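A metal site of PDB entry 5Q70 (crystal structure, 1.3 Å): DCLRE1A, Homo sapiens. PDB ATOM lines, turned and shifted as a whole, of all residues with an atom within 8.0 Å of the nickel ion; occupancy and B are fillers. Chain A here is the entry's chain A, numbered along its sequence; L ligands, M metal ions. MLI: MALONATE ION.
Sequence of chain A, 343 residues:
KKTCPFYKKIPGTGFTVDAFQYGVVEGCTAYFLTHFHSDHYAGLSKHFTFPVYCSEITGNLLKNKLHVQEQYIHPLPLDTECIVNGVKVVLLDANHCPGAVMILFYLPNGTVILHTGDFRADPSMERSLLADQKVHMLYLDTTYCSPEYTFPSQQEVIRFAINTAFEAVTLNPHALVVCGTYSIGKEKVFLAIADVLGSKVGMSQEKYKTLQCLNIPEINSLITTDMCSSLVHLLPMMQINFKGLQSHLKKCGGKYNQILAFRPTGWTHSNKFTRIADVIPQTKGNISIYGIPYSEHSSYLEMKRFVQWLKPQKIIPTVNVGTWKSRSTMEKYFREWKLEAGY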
ATOM      1  N   ASP A  18      10.720   3.320  16.915  1.00  0.00           N
ATOM      2  CA  ASP A  18       9.981   3.862  15.738  1.00  0.00           C
ATOM      3  C   ASP A  18      10.846   3.734  14.404  1.00  0.00           C
ATOM      4  O   ASP A  18      10.930   4.667  13.565  1.00  0.00           O
ATOM      5  CB  ASP A  18       9.473   5.253  15.977  1.00  0.00           C
ATOM      6  CG  ASP A  18       8.498   5.343  17.188  1.00  0.00           C
ATOM      7  OD1 ASP A  18       7.991   4.262  17.652  1.00  0.00           O
ATOM      8  OD2 ASP A  18       8.270   6.517  17.562  1.00  0.00           O
ATOM      9  N   THR A  34       6.234   3.618  19.662  1.00  0.00           N
ATOM     10  CA  THR A  34       5.673   4.538  20.685  1.00  0.00           C
ATOM     11  C   THR A  34       4.127   4.713  20.503  1.00  0.00           C
ATOM     12  O   THR A  34       3.397   4.884  21.471  1.00  0.00           O
ATOM     13  CB  THR A  34       6.339   5.899  20.654  1.00  0.00           C
ATOM     14  OG1 THR A  34       6.166   6.567  19.361  1.00  0.00           O
ATOM     15  CG2 THR A  34       7.845   5.871  21.050  1.00  0.00           C
ATOM     16  N   HIS A  35       3.637   4.679  19.225  1.00  0.00           N
ATOM     17  CA  HIS A  35       2.249   4.978  18.952  1.00  0.00           C
ATOM     18  C   HIS A  35       1.880   4.547  17.539  1.00  0.00           C
ATOM     19  O   HIS A  35       2.766   4.526  16.691  1.00  0.00           O
ATOM     20  CB  HIS A  35       1.840   6.429  19.278  1.00  0.00           C
ATOM     21  CG  HIS A  35       2.407   7.491  18.423  1.00  0.00           C
ATOM     22  ND1 HIS A  35       3.748   7.843  18.360  1.00  0.00           N
ATOM     23  CD2 HIS A  35       1.797   8.373  17.586  1.00  0.00           C
ATOM     24  CE1 HIS A  35       3.905   8.861  17.527  1.00  0.00           C
ATOM     25  NE2 HIS A  35       2.717   9.217  17.079  1.00  0.00           N
ATOM     26  N   PHE A  36       0.577   4.377  17.306  1.00  0.00           N
ATOM     27  CA  PHE A  36       0.085   3.980  15.928  1.00  0.00           C
ATOM     28  C   PHE A  36      -0.186   5.155  15.046  1.00  0.00           C
ATOM     29  O   PHE A  36      -1.401   5.386  14.700  1.00  0.00           O
ATOM     30  CB  PHE A  36      -1.121   3.036  16.127  1.00  0.00           C
ATOM     31  CG  PHE A  36      -1.513   2.267  14.840  1.00  0.00           C
ATOM     32  CD1 PHE A  36      -0.795   1.163  14.513  1.00  0.00           C
ATOM     33  CD2 PHE A  36      -2.630   2.615  14.057  1.00  0.00           C
ATOM     34  CE1 PHE A  36      -1.130   0.431  13.373  1.00  0.00           C
ATOM     35  CE2 PHE A  36      -2.982   1.889  12.944  1.00  0.00           C
ATOM     36  CZ  PHE A  36      -2.263   0.799  12.618  1.00  0.00           C
ATOM     37  N   HIS A  37       0.849   5.883  14.593  1.00  0.00           N
ATOM     38  CA  HIS A  37       0.762   6.901  13.575  1.00  0.00           C
ATOM     39  C   HIS A  37       1.725   6.490  12.409  1.00  0.00           C
ATOM     40  O   HIS A  37       2.849   5.993  12.662  1.00  0.00           O
ATOM     41  CB  HIS A  37       1.124   8.331  14.089  1.00  0.00           C
ATOM     42  CG  HIS A  37      -0.016   9.088  14.759  1.00  0.00           C
ATOM     43  ND1 HIS A  37       0.148  10.247  15.482  1.00  0.00           N
ATOM     44  CD2 HIS A  37      -1.353   8.845  14.743  1.00  0.00           C
ATOM     45  CE1 HIS A  37      -1.037  10.704  15.871  1.00  0.00           C
ATOM     46  NE2 HIS A  37      -1.945   9.849  15.454  1.00  0.00           N
ATOM     47  N   SER A  38       1.311   6.703  11.156  1.00  0.00           N
ATOM     48  CA  SER A  38       1.999   6.093  10.008  1.00  0.00           C
ATOM     49  C   SER A  38       3.414   6.555   9.837  1.00  0.00           C
ATOM     50  O   SER A  38       4.235   5.742   9.345  1.00  0.00           O
ATOM     51  CB  SER A  38       1.147   6.264   8.726  1.00  0.00           C
ATOM     52  OG  SER A  38       1.023   7.643   8.405  1.00  0.00           O
ATOM     53  N   ASP A  39       3.753   7.780  10.188  1.00  0.00           N
ATOM     54  CA  ASP A  39       5.179   8.197  10.072  1.00  0.00           C
ATOM     55  C   ASP A  39       6.064   7.347  11.000  1.00  0.00           C
ATOM     56  O   ASP A  39       7.245   7.155  10.725  1.00  0.00           O
ATOM     57  CB  ASP A  39       5.382   9.666  10.346  1.00  0.00           C
ATOM     58  CG  ASP A  39       5.080  10.601   9.096  1.00  0.00           C
ATOM     59  OD1 ASP A  39       4.791  10.101   7.981  1.00  0.00           O
ATOM     60  OD2 ASP A  39       5.118  11.830   9.318  1.00  0.00           O
ATOM     61  N   HIS A  40       5.491   6.820  12.096  1.00  0.00           N
ATOM     62  CA  HIS A  40       6.241   6.044  13.099  1.00  0.00           C
ATOM     63  C   HIS A  40       6.202   4.561  12.867  1.00  0.00           C
ATOM     64  O   HIS A  40       7.269   3.876  13.040  1.00  0.00           O
ATOM     65  CB  HIS A  40       5.734   6.416  14.549  1.00  0.00           C
ATOM     66  CG  HIS A  40       5.948   7.848  14.858  1.00  0.00           C
ATOM     67  ND1 HIS A  40       6.976   8.327  15.645  1.00  0.00           N
ATOM     68  CD2 HIS A  40       5.294   8.933  14.415  1.00  0.00           C
ATOM     69  CE1 HIS A  40       6.933   9.635  15.664  1.00  0.00           C
ATOM     70  NE2 HIS A  40       5.917  10.032  14.917  1.00  0.00           N
ATOM     71  N   HIS A  96      -0.838  12.003  23.918  1.00  0.00           N
ATOM     72  CA  HIS A  96      -0.844  12.205  22.440  1.00  0.00           C
ATOM     73  C   HIS A  96      -2.137  11.535  21.979  1.00  0.00           C
ATOM     74  O   HIS A  96      -3.194  12.100  22.320  1.00  0.00           O
ATOM     75  CB  HIS A  96       0.467  11.652  21.825  1.00  0.00           C
ATOM     76  CG  HIS A  96       0.658  11.903  20.360  1.00  0.00           C
ATOM     77  ND1 HIS A  96       0.547  13.137  19.764  1.00  0.00           N
ATOM     78  CD2 HIS A  96       0.916  11.039  19.356  1.00  0.00           C
ATOM     79  CE1 HIS A  96       0.779  13.007  18.456  1.00  0.00           C
ATOM     80  NE2 HIS A  96       1.016  11.759  18.187  1.00  0.00           N
ATOM     81  N   CYS A  97      -2.133  10.491  21.200  1.00  0.00           N
ATOM     82  CA  CYS A  97      -3.313   9.774  20.690  1.00  0.00           C
ATOM     83  C   CYS A  97      -3.501   8.532  21.630  1.00  0.00           C
ATOM     84  O   CYS A  97      -2.601   8.190  22.415  1.00  0.00           O
ATOM     85  CB  CYS A  97      -3.118   9.376  19.189  1.00  0.00           C
ATOM     86  SG  CYS A  97      -1.724   8.248  18.956  1.00  0.00           S
ATOM     87  N   ALA A 100      -0.518   5.963  22.973  1.00  0.00           N
ATOM     88  CA  ALA A 100       0.816   6.596  22.783  1.00  0.00           C
ATOM     89  C   ALA A 100       1.545   6.634  24.128  1.00  0.00           C
ATOM     90  O   ALA A 100       0.973   6.979  25.187  1.00  0.00           O
ATOM     91  CB  ALA A 100       0.673   7.983  22.246  1.00  0.00           C
ATOM     92  N   GLY A 117       8.616   9.904  22.480  1.00  0.00           N
ATOM     93  CA  GLY A 117       7.782   9.653  21.334  1.00  0.00           C
ATOM     94  C   GLY A 117       7.205  10.965  20.894  1.00  0.00           C
ATOM     95  O   GLY A 117       7.890  11.976  20.949  1.00  0.00           O
ATOM     96  N   ASP A 118       5.962  10.934  20.391  1.00  0.00           N
ATOM     97  CA  ASP A 118       5.189  12.192  20.232  1.00  0.00           C
ATOM     98  C   ASP A 118       4.396  12.419  21.573  1.00  0.00           C
ATOM     99  O   ASP A 118       3.792  11.482  22.137  1.00  0.00           O
ATOM    100  CB  ASP A 118       4.181  12.096  19.078  1.00  0.00           C
ATOM    101  CG  ASP A 118       4.781  12.246  17.679  1.00  0.00           C
ATOM    102  OD1 ASP A 118       5.939  12.636  17.517  1.00  0.00           O
ATOM    103  OD2 ASP A 118       4.018  12.029  16.726  1.00  0.00           O
ATOM    104  N   PHE A 119       4.394  13.653  22.012  1.00  0.00           N
ATOM    105  CA  PHE A 119       3.735  13.994  23.359  1.00  0.00           C
ATOM    106  C   PHE A 119       3.175  15.401  23.371  1.00  0.00           C
ATOM    107  O   PHE A 119       3.612  16.273  22.634  1.00  0.00           O
ATOM    108  CB  PHE A 119       4.638  13.656  24.567  1.00  0.00           C
ATOM    109  CG  PHE A 119       5.664  14.735  25.042  1.00  0.00           C
ATOM    110  CD1 PHE A 119       5.843  14.934  26.414  1.00  0.00           C
ATOM    111  CD2 PHE A 119       6.468  15.522  24.158  1.00  0.00           C
ATOM    112  CE1 PHE A 119       6.812  15.765  26.892  1.00  0.00           C
ATOM    113  CE2 PHE A 119       7.397  16.459  24.648  1.00  0.00           C
ATOM    114  CZ  PHE A 119       7.553  16.580  26.020  1.00  0.00           C
ATOM    115  N   ASP A 141      10.316  15.245  21.383  1.00  0.00           N
ATOM    116  CA  ASP A 141       9.340  15.683  20.334  1.00  0.00           C
ATOM    117  C   ASP A 141       9.329  17.212  20.331  1.00  0.00           C
ATOM    118  O   ASP A 141       8.704  17.856  21.174  1.00  0.00           O
ATOM    119  CB  ASP A 141       7.924  15.153  20.618  1.00  0.00           C
ATOM    120  CG  ASP A 141       6.869  15.766  19.772  1.00  0.00           C
ATOM    121  OD1 ASP A 141       7.243  16.403  18.741  1.00  0.00           O
ATOM    122  OD2 ASP A 141       5.674  15.615  20.122  1.00  0.00           O
ATOM    123  N   THR A 143       8.244  19.129  17.707  1.00  0.00           N
ATOM    124  CA  THR A 143       7.381  19.568  16.632  1.00  0.00           C
ATOM    125  C   THR A 143       7.110  21.067  16.648  1.00  0.00           C
ATOM    126  O   THR A 143       7.333  21.742  15.559  1.00  0.00           O
ATOM    127  CB  THR A 143       6.007  18.764  16.686  1.00  0.00           C
ATOM    128  OG1 THR A 143       6.191  17.401  16.438  1.00  0.00           O
ATOM    129  CG2 THR A 143       5.070  19.287  15.612  1.00  0.00           C
ATOM    130  N   SER A 183      -6.402   9.697  11.011  1.00  0.00           N
ATOM    131  CA  SER A 183      -5.561   8.859  11.820  1.00  0.00           C
ATOM    132  C   SER A 183      -6.309   8.719  13.149  1.00  0.00           C
ATOM    133  O   SER A 183      -7.335   9.386  13.399  1.00  0.00           O
ATOM    134  CB  SER A 183      -4.193   9.566  12.054  1.00  0.00           C
ATOM    135  OG  SER A 183      -4.353  10.819  12.749  1.00  0.00           O
ATOM    136  N   ILE A 184      -5.769   7.934  14.019  1.00  0.00           N
ATOM    137  CA  ILE A 184      -6.246   7.968  15.413  1.00  0.00           C
ATOM    138  C   ILE A 184      -5.749   9.256  16.123  1.00  0.00           C
ATOM    139  O   ILE A 184      -4.829   9.950  15.632  1.00  0.00           O
ATOM    140  CB  ILE A 184      -5.868   6.737  16.285  1.00  0.00           C
ATOM    141  CG1 ILE A 184      -4.370   6.604  16.475  1.00  0.00           C
ATOM    142  CG2 ILE A 184      -6.458   5.483  15.609  1.00  0.00           C
ATOM    143  CD1 ILE A 184      -3.882   5.629  17.500  1.00  0.00           C
ATOM    144  N   GLU A 296      -2.479  17.682  19.626  1.00  0.00           N
ATOM    145  CA  GLU A 296      -1.903  16.601  20.465  1.00  0.00           C
ATOM    146  C   GLU A 296      -0.349  16.605  20.604  1.00  0.00           C
ATOM    147  O   GLU A 296       0.282  15.615  20.960  1.00  0.00           O
ATOM    148  CB  GLU A 296      -2.430  15.217  20.024  1.00  0.00           C
ATOM    149  CG  GLU A 296      -3.981  15.037  20.373  1.00  0.00           C
ATOM    150  CD  GLU A 296      -4.614  13.688  20.121  1.00  0.00           C
ATOM    151  OE1 GLU A 296      -4.053  12.932  19.241  1.00  0.00           O
ATOM    152  OE2 GLU A 296      -5.733  13.484  20.736  1.00  0.00           O
ATOM    153  N   HIS A 297       0.222  17.754  20.218  1.00  0.00           N
ATOM    154  CA  HIS A 297       1.663  18.062  20.533  1.00  0.00           C
ATOM    155  C   HIS A 297       1.829  19.255  21.479  1.00  0.00           C
ATOM    156  O   HIS A 297       0.990  20.173  21.485  1.00  0.00           O
ATOM    157  CB  HIS A 297       2.464  18.365  19.207  1.00  0.00           C
ATOM    158  CG  HIS A 297       2.571  17.221  18.268  1.00  0.00           C
ATOM    159  ND1 HIS A 297       3.578  16.280  18.317  1.00  0.00           N
ATOM    160  CD2 HIS A 297       1.862  16.926  17.150  1.00  0.00           C
ATOM    161  CE1 HIS A 297       3.443  15.436  17.311  1.00  0.00           C
ATOM    162  NE2 HIS A 297       2.379  15.780  16.640  1.00  0.00           N
HETATM  163  C1  MLI L   1       1.619  12.642  13.229  1.00  0.00           C
HETATM  164  C2  MLI L   1       1.423  13.628  14.364  1.00  0.00           C
HETATM  165  C3  MLI L   1       2.882  11.760  13.385  1.00  0.00           C
HETATM  166  O6  MLI L   1       1.177  14.843  14.229  1.00  0.00           O
HETATM  167  O7  MLI L   1       1.455  13.144  15.481  1.00  0.00           O
HETATM  168  O8  MLI L   1       2.977  10.957  14.341  1.00  0.00           O
HETATM  169  O9  MLI L   1       3.781  11.811  12.502  1.00  0.00           O
HETATM  170 NI    NI M   1       2.057  11.176  16.208  1.00  0.00          NI
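O8 of the ligand is bound to the nickel ion, 2.1 Å away.
The nickel ion is bound by an oxygen (O7) of the ligand, at 2.2 Å.
OD2 of Asp 118 binds the nickel ion.
The nickel ion is bound by ND1 of His 37.
A ring nitrogen (NE2) of His 35 binds the nickel ion (2.2 Å).
The nickel ion is bound by a ring nitrogen (NE2) of His 96 (2.3 Å).
The nickel ion has six donor atoms within binding distance.
OD2 of Asp 118 lies close to NE2 of His 40 (3.3 Å).
O of Ile 184 sits at hydrogen-bond distance from NE2 of His 37.
A ring nitrogen (ND1) of His 35 lies within hydrogen-bond range of the side-chain hydroxyl (OG1) of Thr 34 (2.9 Å).
A ring nitrogen (ND1) of His 96 is in hydrogen-bond range of the backbone carbonyl oxygen of Glu 296.
Within 4 Å of the nickel ion: His 35, His 37, His 96 and Asp 118.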
